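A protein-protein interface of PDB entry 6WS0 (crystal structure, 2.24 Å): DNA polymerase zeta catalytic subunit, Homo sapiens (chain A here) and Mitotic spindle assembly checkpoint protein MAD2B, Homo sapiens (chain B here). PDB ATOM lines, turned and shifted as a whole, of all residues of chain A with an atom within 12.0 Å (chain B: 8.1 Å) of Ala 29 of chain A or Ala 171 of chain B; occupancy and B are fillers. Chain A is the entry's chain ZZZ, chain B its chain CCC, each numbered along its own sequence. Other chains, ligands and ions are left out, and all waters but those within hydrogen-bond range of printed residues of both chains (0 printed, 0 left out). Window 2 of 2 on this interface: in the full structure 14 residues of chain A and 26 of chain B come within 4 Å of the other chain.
O of Val 166 of chain B is in hydrogen-bond range of N of Leu 32 of chain A (2.8 Å).
The backbone carbonyl oxygen (O) of Asn 30 of chain A sits at hydrogen-bond distance from the backbone NH (N) of Thr 168 of chain B.
O of Ile 31 of chain A sits at hydrogen-bond distance from N of Ala 190 of chain B (2.8 Å).
The backbone carbonyl oxygen (O) of Asn 30 of chain A sits close to the backbone carbonyl oxygen (O) of Val 166 of chain B, at 3.5 Å.
The backbone carbonyl oxygen (O) of Glu 170 of chain B sits at hydrogen-bond distance from the side-chain hydroxyl (OG1) of Thr 168 of chain B (3.0 Å).
Among the printed residues, pairs that only touch across the chains: Ala 29 of chain A with Ala 171 of chain B, Ala 29 of chain A with Leu 189 of chain B, Asn 30 of chain A with His 167 of chain B, Ile 31 of chain A with Val 166 of chain B, Ile 31 of chain A with His 167 of chain B, Ile 31 of chain A with Leu 189 of chain B, Leu 32 of chain A with Leu 189 of chain B and Lys 33 of chain A with Ala 190 of chain B.
Ala 29 of chain A touches two residues of chain B.
Of chain A, only Ala 29 comes within 4 Å of Ala 171 of chain B.
Of chain A, only Asn 30 comes within 4 Å of Thr 168 of chain B.
No residue of chain A comes within 4 Å of Ala 172 of chain B.
Of chain A, only Ala 29 (3.7 Å), Ile 31 (3.3 Å) and Leu 32 (3.5 Å) come within 4 Å of Leu 189 of chain B.
Of the printed residues of chain A, Ala 190 of chain B touches Ile 31 and Lys 33.
Of the printed residues of chain B, Ile 31 of chain A touches Val 166 (3.4 Å), His 167 (3.7 Å), Leu 189 (3.3 Å) and Ala 190 (2.8 Å).
The nearest residue of chain A that does not touch Ala 171 of chain B is Asn 30 of chain A (4.3 Å).
The nearest printed residue of chain B that does not touch Leu 32 of chain A is Met 176 of chain B (4.01 Å).
Hydrophobic or aromatic side chains of chain A that line the printed part of chain B: Ile 31 and Leu 32.
Of the 14 printed residues of chain B, 6 touch a printed residue of chain A.
Hydrophobic or aromatic side chains of chain B within 4 Å of the printed part of chain A: Val 166, His 167, Ala 171, Leu 189 and Ala 190.
Among the printed residues, 12 pairs touch across the chains.
Among the printed residues, no Asp or Glu carboxylate lies within 4 Å of a Lys or Arg side-chain nitrogen of the other chain.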
ATOM      1  N   ARG A  27      37.471  -2.367  -7.558  1.00  0.00           N
ATOM      2  CA  ARG A  27      37.092  -2.249  -6.113  1.00  0.00           C
ATOM      3  C   ARG A  27      35.772  -1.472  -5.991  1.00  0.00           C
ATOM      4  O   ARG A  27      35.812  -0.350  -5.450  1.00  0.00           O
ATOM      5  CB  ARG A  27      38.212  -1.558  -5.324  1.00  0.00           C
ATOM      6  CG  ARG A  27      39.438  -2.425  -5.063  1.00  0.00           C
ATOM      7  CD  ARG A  27      40.381  -1.822  -4.033  1.00  0.00           C
ATOM      8  NE  ARG A  27      39.715  -1.435  -2.783  1.00  0.00           N
ATOM      9  CZ  ARG A  27      40.074  -1.802  -1.548  1.00  0.00           C
ATOM     10  NH1 ARG A  27      41.124  -2.585  -1.346  1.00  0.00           N
ATOM     11  NH2 ARG A  27      39.373  -1.366  -0.508  1.00  0.00           N
ATOM     12  N   THR A  28      34.654  -2.060  -6.447  1.00  0.00           N
ATOM     13  CA  THR A  28      33.336  -1.392  -6.664  1.00  0.00           C
ATOM     14  C   THR A  28      32.854  -0.736  -5.362  1.00  0.00           C
ATOM     15  O   THR A  28      33.107  -1.321  -4.276  1.00  0.00           O
ATOM     16  CB  THR A  28      32.288  -2.359  -7.234  1.00  0.00           C
ATOM     17  OG1 THR A  28      32.934  -3.270  -8.123  1.00  0.00           O
ATOM     18  CG2 THR A  28      31.177  -1.642  -7.970  1.00  0.00           C
ATOM     19  N   ALA A  29      32.161   0.409  -5.495  1.00  0.00           N
ATOM     20  CA  ALA A  29      31.988   1.465  -4.463  1.00  0.00           C
ATOM     21  C   ALA A  29      30.497   1.711  -4.179  1.00  0.00           C
ATOM     22  O   ALA A  29      30.028   2.842  -4.355  1.00  0.00           O
ATOM     23  CB  ALA A  29      32.653   2.735  -4.941  1.00  0.00           C
ATOM     24  N   ASN A  30      29.778   0.675  -3.756  1.00  0.00           N
ATOM     25  CA  ASN A  30      28.298   0.668  -3.634  1.00  0.00           C
ATOM     26  C   ASN A  30      27.931   0.347  -2.176  1.00  0.00           C
ATOM     27  O   ASN A  30      26.748  -0.015  -1.877  1.00  0.00           O
ATOM     28  CB  ASN A  30      27.718  -0.333  -4.624  1.00  0.00           C
ATOM     29  CG  ASN A  30      28.114  -1.726  -4.213  1.00  0.00           C
ATOM     30  OD1 ASN A  30      29.307  -2.025  -4.154  1.00  0.00           O
ATOM     31  ND2 ASN A  30      27.128  -2.535  -3.846  1.00  0.00           N
ATOM     32  N   ILE A  31      28.884   0.522  -1.267  1.00  0.00           N
ATOM     33  CA  ILE A  31      28.640   0.189   0.155  1.00  0.00           C
ATOM     34  C   ILE A  31      28.861   1.437   0.984  1.00  0.00           C
ATOM     35  O   ILE A  31      29.987   1.966   0.983  1.00  0.00           O
ATOM     36  CB  ILE A  31      29.466  -1.014   0.622  1.00  0.00           C
ATOM     37  CG1 ILE A  31      29.262  -2.201  -0.325  1.00  0.00           C
ATOM     38  CG2 ILE A  31      29.101  -1.352   2.068  1.00  0.00           C
ATOM     39  CD1 ILE A  31      30.267  -3.331  -0.145  1.00  0.00           C
ATOM     40  N   LEU A  32      27.792   1.880   1.662  1.00  0.00           N
ATOM     41  CA  LEU A  32      27.814   3.139   2.452  1.00  0.00           C
ATOM     42  C   LEU A  32      27.680   2.783   3.936  1.00  0.00           C
ATOM     43  O   LEU A  32      26.944   1.838   4.248  1.00  0.00           O
ATOM     44  CB  LEU A  32      26.690   4.060   1.949  1.00  0.00           C
ATOM     45  CG  LEU A  32      26.928   4.728   0.586  1.00  0.00           C
ATOM     46  CD1 LEU A  32      25.671   5.397   0.064  1.00  0.00           C
ATOM     47  CD2 LEU A  32      28.034   5.773   0.696  1.00  0.00           C
ATOM     48  N   LYS A  33      28.363   3.508   4.810  1.00  0.00           N
ATOM     49  CA  LYS A  33      28.240   3.285   6.266  1.00  0.00           C
ATOM     50  C   LYS A  33      28.453   4.588   7.016  1.00  0.00           C
ATOM     51  O   LYS A  33      29.192   5.475   6.566  1.00  0.00           O
ATOM     52  CB  LYS A  33      29.268   2.260   6.733  1.00  0.00           C
ATOM     53  CG  LYS A  33      30.708   2.737   6.696  1.00  0.00           C
ATOM     54  CD  LYS A  33      31.701   1.677   7.169  1.00  0.00           C
ATOM     55  CE  LYS A  33      31.532   1.315   8.626  1.00  0.00           C
ATOM     56  NZ  LYS A  33      32.102   2.388   9.458  1.00  0.00           N
ATOM     57  N   ASP B  95      16.800   2.007  -4.501  1.00  0.00           N
ATOM     58  CA  ASP B  95      18.253   2.016  -4.822  1.00  0.00           C
ATOM     59  C   ASP B  95      19.099   1.197  -3.812  1.00  0.00           C
ATOM     60  O   ASP B  95      20.345   1.249  -3.906  1.00  0.00           O
ATOM     61  CB  ASP B  95      18.720   3.466  -4.988  1.00  0.00           C
ATOM     62  CG  ASP B  95      18.032   4.200  -6.146  1.00  0.00           C
ATOM     63  OD1 ASP B  95      17.404   3.522  -7.007  1.00  0.00           O
ATOM     64  OD2 ASP B  95      18.095   5.456  -6.168  1.00  0.00           O
ATOM     65  N   VAL B 166      24.914  -0.226   4.048  1.00  0.00           N
ATOM     66  CA  VAL B 166      23.864  -0.054   3.018  1.00  0.00           C
ATOM     67  C   VAL B 166      24.507  -0.336   1.672  1.00  0.00           C
ATOM     68  O   VAL B 166      25.403   0.430   1.293  1.00  0.00           O
ATOM     69  CB  VAL B 166      23.315   1.375   3.050  1.00  0.00           C
ATOM     70  CG1 VAL B 166      22.356   1.568   1.894  1.00  0.00           C
ATOM     71  CG2 VAL B 166      22.668   1.683   4.390  1.00  0.00           C
ATOM     72  N   HIS B 167      24.145  -1.447   1.040  1.00  0.00           N
ATOM     73  CA  HIS B 167      24.632  -1.839  -0.317  1.00  0.00           C
ATOM     74  C   HIS B 167      23.663  -1.265  -1.329  1.00  0.00           C
ATOM     75  O   HIS B 167      22.484  -1.611  -1.269  1.00  0.00           O
ATOM     76  CB  HIS B 167      24.730  -3.366  -0.499  1.00  0.00           C
ATOM     77  CG  HIS B 167      25.756  -4.027   0.367  1.00  0.00           C
ATOM     78  ND1 HIS B 167      25.812  -3.801   1.749  1.00  0.00           N
ATOM     79  CD2 HIS B 167      26.744  -4.925   0.075  1.00  0.00           C
ATOM     80  CE1 HIS B 167      26.816  -4.516   2.264  1.00  0.00           C
ATOM     81  NE2 HIS B 167      27.390  -5.226   1.255  1.00  0.00           N
ATOM     82  N   THR B 168      24.127  -0.397  -2.209  1.00  0.00           N
ATOM     83  CA  THR B 168      23.254   0.214  -3.247  1.00  0.00           C
ATOM     84  C   THR B 168      23.209  -0.724  -4.461  1.00  0.00           C
ATOM     85  O   THR B 168      24.210  -1.422  -4.706  1.00  0.00           O
ATOM     86  CB  THR B 168      23.764   1.628  -3.569  1.00  0.00           C
ATOM     87  OG1 THR B 168      25.153   1.575  -3.934  1.00  0.00           O
ATOM     88  CG2 THR B 168      23.563   2.538  -2.380  1.00  0.00           C
ATOM     89  N   ARG B 169      22.125  -0.694  -5.224  1.00  0.00           N
ATOM     90  CA  ARG B 169      21.985  -1.458  -6.497  1.00  0.00           C
ATOM     91  C   ARG B 169      23.055  -1.031  -7.499  1.00  0.00           C
ATOM     92  O   ARG B 169      23.580  -1.896  -8.215  1.00  0.00           O
ATOM     93  CB  ARG B 169      20.617  -1.226  -7.137  1.00  0.00           C
ATOM     94  CG  ARG B 169      19.475  -1.666  -6.239  1.00  0.00           C
ATOM     95  CD  ARG B 169      18.264  -2.069  -7.018  1.00  0.00           C
ATOM     96  NE  ARG B 169      17.233  -2.494  -6.089  1.00  0.00           N
ATOM     97  CZ  ARG B 169      17.202  -3.657  -5.432  1.00  0.00           C
ATOM     98  NH1 ARG B 169      18.160  -4.560  -5.571  1.00  0.00           N
ATOM     99  NH2 ARG B 169      16.190  -3.902  -4.624  1.00  0.00           N
ATOM    100  N   GLU B 170      23.299   0.269  -7.626  1.00  0.00           N
ATOM    101  CA  GLU B 170      24.400   0.788  -8.478  1.00  0.00           C
ATOM    102  C   GLU B 170      25.081   1.894  -7.682  1.00  0.00           C
ATOM    103  O   GLU B 170      24.449   2.428  -6.734  1.00  0.00           O
ATOM    104  CB  GLU B 170      23.918   1.215  -9.876  1.00  0.00           C
ATOM    105  CG  GLU B 170      22.729   2.171  -9.883  1.00  0.00           C
ATOM    106  CD  GLU B 170      22.398   2.797 -11.235  1.00  0.00           C
ATOM    107  OE1 GLU B 170      23.057   2.427 -12.235  1.00  0.00           O
ATOM    108  OE2 GLU B 170      21.503   3.680 -11.281  1.00  0.00           O
ATOM    109  N   ALA B 171      26.361   2.088  -7.969  1.00  0.00           N
ATOM    110  CA  ALA B 171      27.181   3.187  -7.435  1.00  0.00           C
ATOM    111  C   ALA B 171      26.675   4.467  -8.102  1.00  0.00           C
ATOM    112  O   ALA B 171      26.889   4.611  -9.296  1.00  0.00           O
ATOM    113  CB  ALA B 171      28.624   2.899  -7.738  1.00  0.00           C
ATOM    114  N   ALA B 172      25.921   5.297  -7.391  1.00  0.00           N
ATOM    115  CA  ALA B 172      25.296   6.500  -7.975  1.00  0.00           C
ATOM    116  C   ALA B 172      25.472   7.678  -7.017  1.00  0.00           C
ATOM    117  O   ALA B 172      25.232   7.542  -5.822  1.00  0.00           O
ATOM    118  CB  ALA B 172      23.843   6.262  -8.317  1.00  0.00           C
ATOM    119  N   THR B 173      25.994   8.754  -7.587  1.00  0.00           N
ATOM    120  CA  THR B 173      26.141  10.107  -7.006  1.00  0.00           C
ATOM    121  C   THR B 173      24.873  10.409  -6.214  1.00  0.00           C
ATOM    122  O   THR B 173      25.022  10.785  -5.050  1.00  0.00           O
ATOM    123  CB  THR B 173      26.554  11.060  -8.140  1.00  0.00           C
ATOM    124  OG1 THR B 173      27.975  10.902  -8.215  1.00  0.00           O
ATOM    125  CG2 THR B 173      26.219  12.510  -7.902  1.00  0.00           C
ATOM    126  N   ARG B 174      23.699  10.112  -6.773  1.00  0.00           N
ATOM    127  CA  ARG B 174      22.404  10.486  -6.154  1.00  0.00           C
ATOM    128  C   ARG B 174      22.298   9.781  -4.794  1.00  0.00           C
ATOM    129  O   ARG B 174      21.787  10.391  -3.857  1.00  0.00           O
ATOM    130  CB  ARG B 174      21.211  10.185  -7.069  1.00  0.00           C
ATOM    131  CG  ARG B 174      20.666   8.755  -6.968  1.00  0.00           C
ATOM    132  CD  ARG B 174      19.634   8.357  -8.045  1.00  0.00           C
ATOM    133  NE  ARG B 174      19.547   6.907  -8.244  1.00  0.00           N
ATOM    134  CZ  ARG B 174      20.263   6.196  -9.115  1.00  0.00           C
ATOM    135  NH1 ARG B 174      21.114   6.783  -9.947  1.00  0.00           N
ATOM    136  NH2 ARG B 174      20.125   4.883  -9.155  1.00  0.00           N
ATOM    137  N   ASN B 175      22.798   8.557  -4.669  1.00  0.00           N
ATOM    138  CA  ASN B 175      22.681   7.802  -3.399  1.00  0.00           C
ATOM    139  C   ASN B 175      23.268   8.613  -2.238  1.00  0.00           C
ATOM    140  O   ASN B 175      22.642   8.697  -1.188  1.00  0.00           O
ATOM    141  CB  ASN B 175      23.338   6.423  -3.499  1.00  0.00           C
ATOM    142  CG  ASN B 175      22.468   5.490  -4.306  1.00  0.00           C
ATOM    143  OD1 ASN B 175      21.251   5.659  -4.293  1.00  0.00           O
ATOM    144  ND2 ASN B 175      23.084   4.563  -5.032  1.00  0.00           N
ATOM    145  N   MET B 176      24.441   9.168  -2.441  1.00  0.00           N
ATOM    146  CA  MET B 176      25.248   9.813  -1.387  1.00  0.00           C
ATOM    147  C   MET B 176      24.776  11.258  -1.166  1.00  0.00           C
ATOM    148  O   MET B 176      24.740  11.685  -0.021  1.00  0.00           O
ATOM    149  CB  MET B 176      26.681   9.745  -1.883  1.00  0.00           C
ATOM    150  CG  MET B 176      27.697  10.096  -0.908  1.00  0.00           C
ATOM    151  SD  MET B 176      29.114   9.070  -1.313  1.00  0.00           S
ATOM    152  CE  MET B 176      30.075   9.498   0.134  1.00  0.00           C
ATOM    153  N   LEU B 189      32.053   5.757   2.106  1.00  0.00           N
ATOM    154  CA  LEU B 189      32.100   4.495   1.335  1.00  0.00           C
ATOM    155  C   LEU B 189      32.946   3.517   2.137  1.00  0.00           C
ATOM    156  O   LEU B 189      34.035   3.900   2.553  1.00  0.00           O
ATOM    157  CB  LEU B 189      32.667   4.826  -0.035  1.00  0.00           C
ATOM    158  CG  LEU B 189      31.783   5.791  -0.815  1.00  0.00           C
ATOM    159  CD1 LEU B 189      32.562   6.544  -1.889  1.00  0.00           C
ATOM    160  CD2 LEU B 189      30.649   5.027  -1.451  1.00  0.00           C
ATOM    161  N   ALA B 190      32.407   2.337   2.422  1.00  0.00           N
ATOM    162  CA  ALA B 190      33.018   1.330   3.327  1.00  0.00           C
ATOM    163  C   ALA B 190      34.251   0.739   2.642  1.00  0.00           C
ATOM    164  O   ALA B 190      34.159   0.541   1.410  1.00  0.00           O
ATOM    165  CB  ALA B 190      31.984   0.261   3.594  1.00  0.00           C
